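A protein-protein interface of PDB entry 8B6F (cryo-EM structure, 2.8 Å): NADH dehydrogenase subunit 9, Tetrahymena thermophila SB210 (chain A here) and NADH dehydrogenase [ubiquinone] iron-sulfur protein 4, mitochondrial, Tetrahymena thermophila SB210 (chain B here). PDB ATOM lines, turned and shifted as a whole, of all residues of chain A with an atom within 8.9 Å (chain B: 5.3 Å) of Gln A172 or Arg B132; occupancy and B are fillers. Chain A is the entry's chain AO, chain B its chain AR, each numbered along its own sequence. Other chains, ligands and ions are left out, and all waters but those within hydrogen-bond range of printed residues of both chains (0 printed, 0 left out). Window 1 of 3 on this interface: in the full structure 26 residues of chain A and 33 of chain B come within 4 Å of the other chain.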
ATOM      1  N   GLU A 164      27.071  28.964  14.401  1.00  0.00           N
ATOM      2  CA  GLU A 164      26.049  27.929  14.345  1.00  0.00           C
ATOM      3  C   GLU A 164      26.659  26.667  13.758  1.00  0.00           C
ATOM      4  O   GLU A 164      27.723  26.702  13.133  1.00  0.00           O
ATOM      5  CB  GLU A 164      24.842  28.376  13.515  1.00  0.00           C
ATOM      6  CG  GLU A 164      25.191  28.771  12.091  1.00  0.00           C
ATOM      7  CD  GLU A 164      23.972  29.153  11.280  1.00  0.00           C
ATOM      8  OE1 GLU A 164      22.875  29.239  11.867  1.00  0.00           O
ATOM      9  OE2 GLU A 164      24.111  29.366  10.058  1.00  0.00           O
ATOM     10  N   ASN A 165      25.966  25.551  13.968  1.00  0.00           N
ATOM     11  CA  ASN A 165      26.347  24.248  13.425  1.00  0.00           C
ATOM     12  C   ASN A 165      25.115  23.667  12.743  1.00  0.00           C
ATOM     13  O   ASN A 165      24.420  22.813  13.310  1.00  0.00           O
ATOM     14  CB  ASN A 165      26.876  23.324  14.521  1.00  0.00           C
ATOM     15  CG  ASN A 165      27.971  23.967  15.344  1.00  0.00           C
ATOM     16  OD1 ASN A 165      27.910  23.989  16.572  1.00  0.00           O
ATOM     17  ND2 ASN A 165      28.981  24.502  14.669  1.00  0.00           N
ATOM     18  N   PRO A 166      24.807  24.118  11.526  1.00  0.00           N
ATOM     19  CA  PRO A 166      23.516  23.752  10.919  1.00  0.00           C
ATOM     20  C   PRO A 166      23.315  22.261  10.716  1.00  0.00           C
ATOM     21  O   PRO A 166      22.175  21.789  10.802  1.00  0.00           O
ATOM     22  CB  PRO A 166      23.539  24.503   9.580  1.00  0.00           C
ATOM     23  CG  PRO A 166      24.977  24.719   9.287  1.00  0.00           C
ATOM     24  CD  PRO A 166      25.641  24.914  10.612  1.00  0.00           C
ATOM     25  N   MET A 167      24.374  21.500  10.442  1.00  0.00           N
ATOM     26  CA  MET A 167      24.198  20.098  10.084  1.00  0.00           C
ATOM     27  C   MET A 167      23.813  19.221  11.266  1.00  0.00           C
ATOM     28  O   MET A 167      23.485  18.049  11.058  1.00  0.00           O
ATOM     29  CB  MET A 167      25.471  19.563   9.433  1.00  0.00           C
ATOM     30  CG  MET A 167      25.708  20.116   8.040  1.00  0.00           C
ATOM     31  SD  MET A 167      24.408  19.656   6.878  1.00  0.00           S
ATOM     32  CE  MET A 167      24.767  20.757   5.513  1.00  0.00           C
ATOM     33  N   LEU A 168      23.851  19.743  12.487  1.00  0.00           N
ATOM     34  CA  LEU A 168      23.357  18.984  13.627  1.00  0.00           C
ATOM     35  C   LEU A 168      21.858  18.749  13.488  1.00  0.00           C
ATOM     36  O   LEU A 168      21.117  19.622  13.032  1.00  0.00           O
ATOM     37  CB  LEU A 168      23.659  19.723  14.929  1.00  0.00           C
ATOM     38  CG  LEU A 168      25.138  19.872  15.295  1.00  0.00           C
ATOM     39  CD1 LEU A 168      25.292  20.712  16.549  1.00  0.00           C
ATOM     40  CD2 LEU A 168      25.794  18.514  15.482  1.00  0.00           C
ATOM     41  N   LYS A 169      21.413  17.558  13.890  1.00  0.00           N
ATOM     42  CA  LYS A 169      20.006  17.202  13.739  1.00  0.00           C
ATOM     43  C   LYS A 169      19.089  18.116  14.539  1.00  0.00           C
ATOM     44  O   LYS A 169      17.904  18.227  14.209  1.00  0.00           O
ATOM     45  CB  LYS A 169      19.782  15.748  14.160  1.00  0.00           C
ATOM     46  CG  LYS A 169      20.374  14.722  13.204  1.00  0.00           C
ATOM     47  CD  LYS A 169      19.663  14.739  11.858  1.00  0.00           C
ATOM     48  CE  LYS A 169      20.235  13.695  10.917  1.00  0.00           C
ATOM     49  NZ  LYS A 169      19.583  13.749   9.579  1.00  0.00           N
ATOM     50  N   GLU A 170      19.602  18.765  15.584  1.00  0.00           N
ATOM     51  CA  GLU A 170      18.778  19.694  16.349  1.00  0.00           C
ATOM     52  C   GLU A 170      18.399  20.910  15.512  1.00  0.00           C
ATOM     53  O   GLU A 170      17.296  21.448  15.650  1.00  0.00           O
ATOM     54  CB  GLU A 170      19.513  20.129  17.616  1.00  0.00           C
ATOM     55  CG  GLU A 170      20.818  20.865  17.351  1.00  0.00           C
ATOM     56  CD  GLU A 170      21.511  21.289  18.626  1.00  0.00           C
ATOM     57  OE1 GLU A 170      20.984  20.989  19.717  1.00  0.00           O
ATOM     58  OE2 GLU A 170      22.582  21.924  18.541  1.00  0.00           O
ATOM     59  N   PHE A 171      19.301  21.356  14.644  1.00  0.00           N
ATOM     60  CA  PHE A 171      19.063  22.553  13.856  1.00  0.00           C
ATOM     61  C   PHE A 171      17.955  22.316  12.837  1.00  0.00           C
ATOM     62  O   PHE A 171      17.781  21.211  12.317  1.00  0.00           O
ATOM     63  CB  PHE A 171      20.347  22.976  13.145  1.00  0.00           C
ATOM     64  CG  PHE A 171      20.346  24.402  12.691  1.00  0.00           C
ATOM     65  CD1 PHE A 171      20.703  25.417  13.561  1.00  0.00           C
ATOM     66  CD2 PHE A 171      20.004  24.729  11.391  1.00  0.00           C
ATOM     67  CE1 PHE A 171      20.711  26.731  13.146  1.00  0.00           C
ATOM     68  CE2 PHE A 171      20.010  26.042  10.971  1.00  0.00           C
ATOM     69  CZ  PHE A 171      20.363  27.045  11.850  1.00  0.00           C
ATOM     70  N   GLN A 172      17.202  23.375  12.555  1.00  0.00           N
ATOM     71  CA  GLN A 172      16.104  23.335  11.602  1.00  0.00           C
ATOM     72  C   GLN A 172      16.563  23.898  10.263  1.00  0.00           C
ATOM     73  O   GLN A 172      17.308  24.880  10.215  1.00  0.00           O
ATOM     74  CB  GLN A 172      14.910  24.134  12.123  1.00  0.00           C
ATOM     75  CG  GLN A 172      14.378  23.645  13.463  1.00  0.00           C
ATOM     76  CD  GLN A 172      13.717  22.287  13.373  1.00  0.00           C
ATOM     77  OE1 GLN A 172      13.358  21.829  12.291  1.00  0.00           O
ATOM     78  NE2 GLN A 172      13.552  21.633  14.516  1.00  0.00           N
ATOM     79  N   SER A 173      16.108  23.272   9.175  1.00  0.00           N
ATOM     80  CA  SER A 173      16.556  23.681   7.848  1.00  0.00           C
ATOM     81  C   SER A 173      16.235  25.141   7.566  1.00  0.00           C
ATOM     82  O   SER A 173      16.990  25.814   6.857  1.00  0.00           O
ATOM     83  CB  SER A 173      15.916  22.793   6.780  1.00  0.00           C
ATOM     84  OG  SER A 173      16.328  21.445   6.922  1.00  0.00           O
ATOM     85  N   GLU A 174      15.126  25.650   8.105  1.00  0.00           N
ATOM     86  CA  GLU A 174      14.737  27.031   7.848  1.00  0.00           C
ATOM     87  C   GLU A 174      15.642  28.039   8.538  1.00  0.00           C
ATOM     88  O   GLU A 174      15.531  29.236   8.253  1.00  0.00           O
ATOM     89  CB  GLU A 174      13.291  27.265   8.289  1.00  0.00           C
ATOM     90  CG  GLU A 174      12.249  26.579   7.416  1.00  0.00           C
ATOM     91  CD  GLU A 174      12.143  25.091   7.681  1.00  0.00           C
ATOM     92  OE1 GLU A 174      12.551  24.648   8.774  1.00  0.00           O
ATOM     93  OE2 GLU A 174      11.647  24.363   6.797  1.00  0.00           O
ATOM     94  N   GLY A 175      16.524  27.599   9.426  1.00  0.00           N
ATOM     95  CA  GLY A 175      17.406  28.514  10.112  1.00  0.00           C
ATOM     96  C   GLY A 175      16.720  29.221  11.266  1.00  0.00           C
ATOM     97  O   GLY A 175      15.593  28.908  11.656  1.00  0.00           O
ATOM     98  N   THR A 176      17.435  30.203  11.819  1.00  0.00           N
ATOM     99  CA  THR A 176      16.950  30.975  12.951  1.00  0.00           C
ATOM    100  C   THR A 176      16.815  32.466  12.676  1.00  0.00           C
ATOM    101  O   THR A 176      16.246  33.175  13.510  1.00  0.00           O
ATOM    102  CB  THR A 176      17.875  30.782  14.166  1.00  0.00           C
ATOM    103  OG1 THR A 176      19.228  31.076  13.799  1.00  0.00           O
ATOM    104  CG2 THR A 176      17.790  29.353  14.680  1.00  0.00           C
ATOM    105  N   GLN A 177      17.311  32.965  11.545  1.00  0.00           N
ATOM    106  CA  GLN A 177      17.207  34.383  11.236  1.00  0.00           C
ATOM    107  C   GLN A 177      17.258  34.573   9.729  1.00  0.00           C
ATOM    108  O   GLN A 177      17.847  33.766   9.005  1.00  0.00           O
ATOM    109  CB  GLN A 177      18.323  35.185  11.919  1.00  0.00           C
ATOM    110  CG  GLN A 177      19.724  34.784  11.494  1.00  0.00           C
ATOM    111  CD  GLN A 177      20.793  35.412  12.364  1.00  0.00           C
ATOM    112  OE1 GLN A 177      20.566  35.694  13.537  1.00  0.00           O
ATOM    113  NE2 GLN A 177      21.969  35.627  11.791  1.00  0.00           N
ATOM    114  N   ASN A 193      13.368  35.021  12.306  1.00  0.00           N
ATOM    115  CA  ASN A 193      12.969  34.240  11.144  1.00  0.00           C
ATOM    116  C   ASN A 193      11.496  33.864  11.226  1.00  0.00           C
ATOM    117  O   ASN A 193      11.041  33.334  12.244  1.00  0.00           O
ATOM    118  CB  ASN A 193      13.831  32.980  11.037  1.00  0.00           C
ATOM    119  CG  ASN A 193      13.538  32.180   9.796  1.00  0.00           C
ATOM    120  OD1 ASN A 193      12.947  32.684   8.845  1.00  0.00           O
ATOM    121  ND2 ASN A 193      13.959  30.922   9.791  1.00  0.00           N
ATOM    122  N   THR A 195       8.845  31.827   8.447  1.00  0.00           N
ATOM    123  CA  THR A 195       8.897  31.107   7.180  1.00  0.00           C
ATOM    124  C   THR A 195       7.543  30.532   6.792  1.00  0.00           C
ATOM    125  O   THR A 195       6.531  30.815   7.441  1.00  0.00           O
ATOM    126  CB  THR A 195       9.935  29.986   7.252  1.00  0.00           C
ATOM    127  OG1 THR A 195       9.585  29.074   8.300  1.00  0.00           O
ATOM    128  CG2 THR A 195      11.311  30.562   7.526  1.00  0.00           C
ATOM    129  N   VAL A 196       7.518  29.727   5.733  1.00  0.00           N
ATOM    130  CA  VAL A 196       6.298  29.132   5.201  1.00  0.00           C
ATOM    131  C   VAL A 196       6.335  27.638   5.481  1.00  0.00           C
ATOM    132  O   VAL A 196       7.351  26.980   5.232  1.00  0.00           O
ATOM    133  CB  VAL A 196       6.157  29.382   3.689  1.00  0.00           C
ATOM    134  CG1 VAL A 196       4.702  29.258   3.264  1.00  0.00           C
ATOM    135  CG2 VAL A 196       6.749  30.725   3.300  1.00  0.00           C
ATOM    136  N   GLU A 197       5.232  27.106   5.998  1.00  0.00           N
ATOM    137  CA  GLU A 197       5.085  25.679   6.246  1.00  0.00           C
ATOM    138  C   GLU A 197       4.121  25.106   5.219  1.00  0.00           C
ATOM    139  O   GLU A 197       2.972  25.550   5.126  1.00  0.00           O
ATOM    140  CB  GLU A 197       4.581  25.416   7.666  1.00  0.00           C
ATOM    141  CG  GLU A 197       4.515  23.940   8.025  1.00  0.00           C
ATOM    142  CD  GLU A 197       3.970  23.703   9.418  1.00  0.00           C
ATOM    143  OE1 GLU A 197       3.647  24.692  10.109  1.00  0.00           O
ATOM    144  OE2 GLU A 197       3.862  22.525   9.823  1.00  0.00           O
ATOM    145  N   LEU B 107      10.965  13.924  20.984  1.00  0.00           N
ATOM    146  CA  LEU B 107      11.015  15.162  21.746  1.00  0.00           C
ATOM    147  C   LEU B 107      10.360  16.253  20.916  1.00  0.00           C
ATOM    148  O   LEU B 107      10.752  16.485  19.767  1.00  0.00           O
ATOM    149  CB  LEU B 107      12.463  15.525  22.091  1.00  0.00           C
ATOM    150  CG  LEU B 107      12.763  16.731  22.990  1.00  0.00           C
ATOM    151  CD1 LEU B 107      14.193  16.655  23.485  1.00  0.00           C
ATOM    152  CD2 LEU B 107      12.546  18.061  22.287  1.00  0.00           C
ATOM    153  N   THR B 128      10.564  29.144  13.810  1.00  0.00           N
ATOM    154  CA  THR B 128      10.928  27.994  12.999  1.00  0.00           C
ATOM    155  C   THR B 128      11.572  26.878  13.807  1.00  0.00           C
ATOM    156  O   THR B 128      11.981  25.869  13.228  1.00  0.00           O
ATOM    157  CB  THR B 128      11.874  28.425  11.874  1.00  0.00           C
ATOM    158  OG1 THR B 128      13.050  29.023  12.432  1.00  0.00           O
ATOM    159  CG2 THR B 128      11.185  29.423  10.962  1.00  0.00           C
ATOM    160  N   PHE B 129      11.674  27.033  15.128  1.00  0.00           N
ATOM    161  CA  PHE B 129      12.358  26.039  15.945  1.00  0.00           C
ATOM    162  C   PHE B 129      11.504  24.796  16.167  1.00  0.00           C
ATOM    163  O   PHE B 129      12.032  23.679  16.208  1.00  0.00           O
ATOM    164  CB  PHE B 129      12.762  26.651  17.285  1.00  0.00           C
ATOM    165  CG  PHE B 129      13.472  25.694  18.193  1.00  0.00           C
ATOM    166  CD1 PHE B 129      14.792  25.351  17.957  1.00  0.00           C
ATOM    167  CD2 PHE B 129      12.824  25.142  19.283  1.00  0.00           C
ATOM    168  CE1 PHE B 129      15.450  24.468  18.788  1.00  0.00           C
ATOM    169  CE2 PHE B 129      13.477  24.258  20.117  1.00  0.00           C
ATOM    170  CZ  PHE B 129      14.793  23.922  19.870  1.00  0.00           C
ATOM    171  N   SER B 130      10.189  24.962  16.312  1.00  0.00           N
ATOM    172  CA  SER B 130       9.298  23.872  16.691  1.00  0.00           C
ATOM    173  C   SER B 130       8.558  23.277  15.498  1.00  0.00           C
ATOM    174  O   SER B 130       7.407  22.849  15.636  1.00  0.00           O
ATOM    175  CB  SER B 130       8.293  24.356  17.737  1.00  0.00           C
ATOM    176  OG  SER B 130       8.951  24.851  18.888  1.00  0.00           O
ATOM    177  N   LYS B 131       9.191  23.239  14.325  1.00  0.00           N
ATOM    178  CA  LYS B 131       8.530  22.668  13.157  1.00  0.00           C
ATOM    179  C   LYS B 131       8.677  21.151  13.120  1.00  0.00           C
ATOM    180  O   LYS B 131       7.696  20.433  12.902  1.00  0.00           O
ATOM    181  CB  LYS B 131       9.092  23.288  11.877  1.00  0.00           C
ATOM    182  CG  LYS B 131       8.159  23.149  10.685  1.00  0.00           C
ATOM    183  CD  LYS B 131       8.825  23.569   9.385  1.00  0.00           C
ATOM    184  CE  LYS B 131       9.768  22.499   8.862  1.00  0.00           C
ATOM    185  NZ  LYS B 131       9.052  21.236   8.529  1.00  0.00           N
ATOM    186  N   ARG B 132       9.889  20.649  13.335  1.00  0.00           N
ATOM    187  CA  ARG B 132      10.178  19.223  13.279  1.00  0.00           C
ATOM    188  C   ARG B 132      10.466  18.692  14.675  1.00  0.00           C
ATOM    189  O   ARG B 132      11.069  19.383  15.501  1.00  0.00           O
ATOM    190  CB  ARG B 132      11.377  18.937  12.375  1.00  0.00           C
ATOM    191  CG  ARG B 132      11.259  19.500  10.973  1.00  0.00           C
ATOM    192  CD  ARG B 132      12.534  19.251  10.183  1.00  0.00           C
ATOM    193  NE  ARG B 132      12.467  19.826   8.846  1.00  0.00           N
ATOM    194  CZ  ARG B 132      12.767  21.083   8.550  1.00  0.00           C
ATOM    195  NH1 ARG B 132      13.152  21.942   9.480  1.00  0.00           N
ATOM    196  NH2 ARG B 132      12.673  21.492   7.288  1.00  0.00           N
ATOM    197  N   ASN B 133      10.031  17.464  14.932  1.00  0.00           N
ATOM    198  CA  ASN B 133      10.341  16.805  16.188  1.00  0.00           C
ATOM    199  C   ASN B 133      11.759  16.250  16.163  1.00  0.00           C
ATOM    200  O   ASN B 133      12.361  16.053  15.104  1.00  0.00           O
ATOM    201  CB  ASN B 133       9.356  15.670  16.463  1.00  0.00           C
ATOM    202  CG  ASN B 133       7.924  16.147  16.536  1.00  0.00           C
ATOM    203  OD1 ASN B 133       7.654  17.282  16.925  1.00  0.00           O
ATOM    204  ND2 ASN B 133       6.994  15.278  16.162  1.00  0.00           N
ATOM    205  N   HIS B 134      12.293  16.002  17.352  1.00  0.00           N
ATOM    206  CA  HIS B 134      13.591  15.366  17.506  1.00  0.00           C
ATOM    207  C   HIS B 134      13.379  13.924  17.939  1.00  0.00           C
ATOM    208  O   HIS B 134      12.390  13.600  18.600  1.00  0.00           O
ATOM    209  CB  HIS B 134      14.450  16.108  18.532  1.00  0.00           C
ATOM    210  CG  HIS B 134      14.724  17.533  18.171  1.00  0.00           C
ATOM    211  ND1 HIS B 134      13.726  18.426  17.846  1.00  0.00           N
ATOM    212  CD2 HIS B 134      15.886  18.221  18.080  1.00  0.00           C
ATOM    213  CE1 HIS B 134      14.261  19.602  17.571  1.00  0.00           C
ATOM    214  NE2 HIS B 134      15.570  19.505  17.705  1.00  0.00           N
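The backbone carbonyl oxygen of Gly A175 is in hydrogen-bond range of the side-chain hydroxyl of Thr B128, 2.7 Å away. N of Ser A173 lies close to NH1 of Arg B132. NE2 of His B134 is in hydrogen-bond range of O of Glu A170. The guanidinium group of Arg B132 lies within hydrogen-bond range of the side-chain amide oxygen of Gln A172 (2.8 Å). The side-chain amide nitrogen of Gln A172 is in hydrogen-bond range of the backbone carbonyl oxygen of Phe B129 (3.1 Å). The side-chain carboxylate (OE1) of Glu A174 is in salt-bridge range of the guanidinium group (NH1) of Arg B132, at 2.9 Å. The side-chain amide nitrogen (ND2) of Asn A193 sits close to the side-chain hydroxyl (OG1) of Thr B128 (3.4 Å).
The backbone carbonyl oxygen of Glu A174 sits at hydrogen-bond distance from the side-chain amide nitrogen of Asn A193. N of Leu B107 is in hydrogen-bond range of O of His B134, at 2.8 Å. ND2 of Asn A193 sits at hydrogen-bond distance from O of Gly A175, 3.2 Å away.
Gln A172 touches Thr B128 (CG to O, 3.3 Å). NE2 of Gln A172 touches CE1 of His B134, 3.7 Å away. Lys B131 touches Glu A174. CG2 of Thr B128 touches OG1 of Thr A195 (3.1 Å).
Gln A172 touches just these residues of chain B: Thr B128 (3.3 Å), Phe B129 (3.1 Å), Arg B132 (2.8 Å) and His B134 (3.7 Å). Of the printed residues of chain A, Arg B132 touches Gln A172 (2.8 Å), Ser A173 (3.3 Å) and Glu A174 (2.9 Å). Lys B131 touches just one residue of chain A: Glu A174. Of the printed residues of chain B, Gly A175 touches Thr B128 (2.7 Å). Of the printed residues of chain B, Glu A170 touches His B134 (3.3 Å). Printed residues of chain A within 4 Å of Phe B129: Gln A172 (3.1 Å). Ser B130 touches none of the printed residues of chain A. Asn A165 touches none of the printed residues of chain B. The nearest residue of chain B that does not touch Gln A172 is Lys B131 (4.5 Å). The nearest printed residue of chain A that does not touch Phe B129 is Glu A170 (4.7 Å).
Of the 18 printed residues of chain A, 7 touch a printed residue of chain B. Printed residues of chain A that touch a printed residue of chain B: Glu A170, Gln A172, Ser A173, Glu A174, Gly A175, Asn A193 and Thr A195. Hydrophobic or aromatic side chains of chain B that line the printed part of chain A: His B134. Among the printed residues, 11 pairs touch across the chains.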
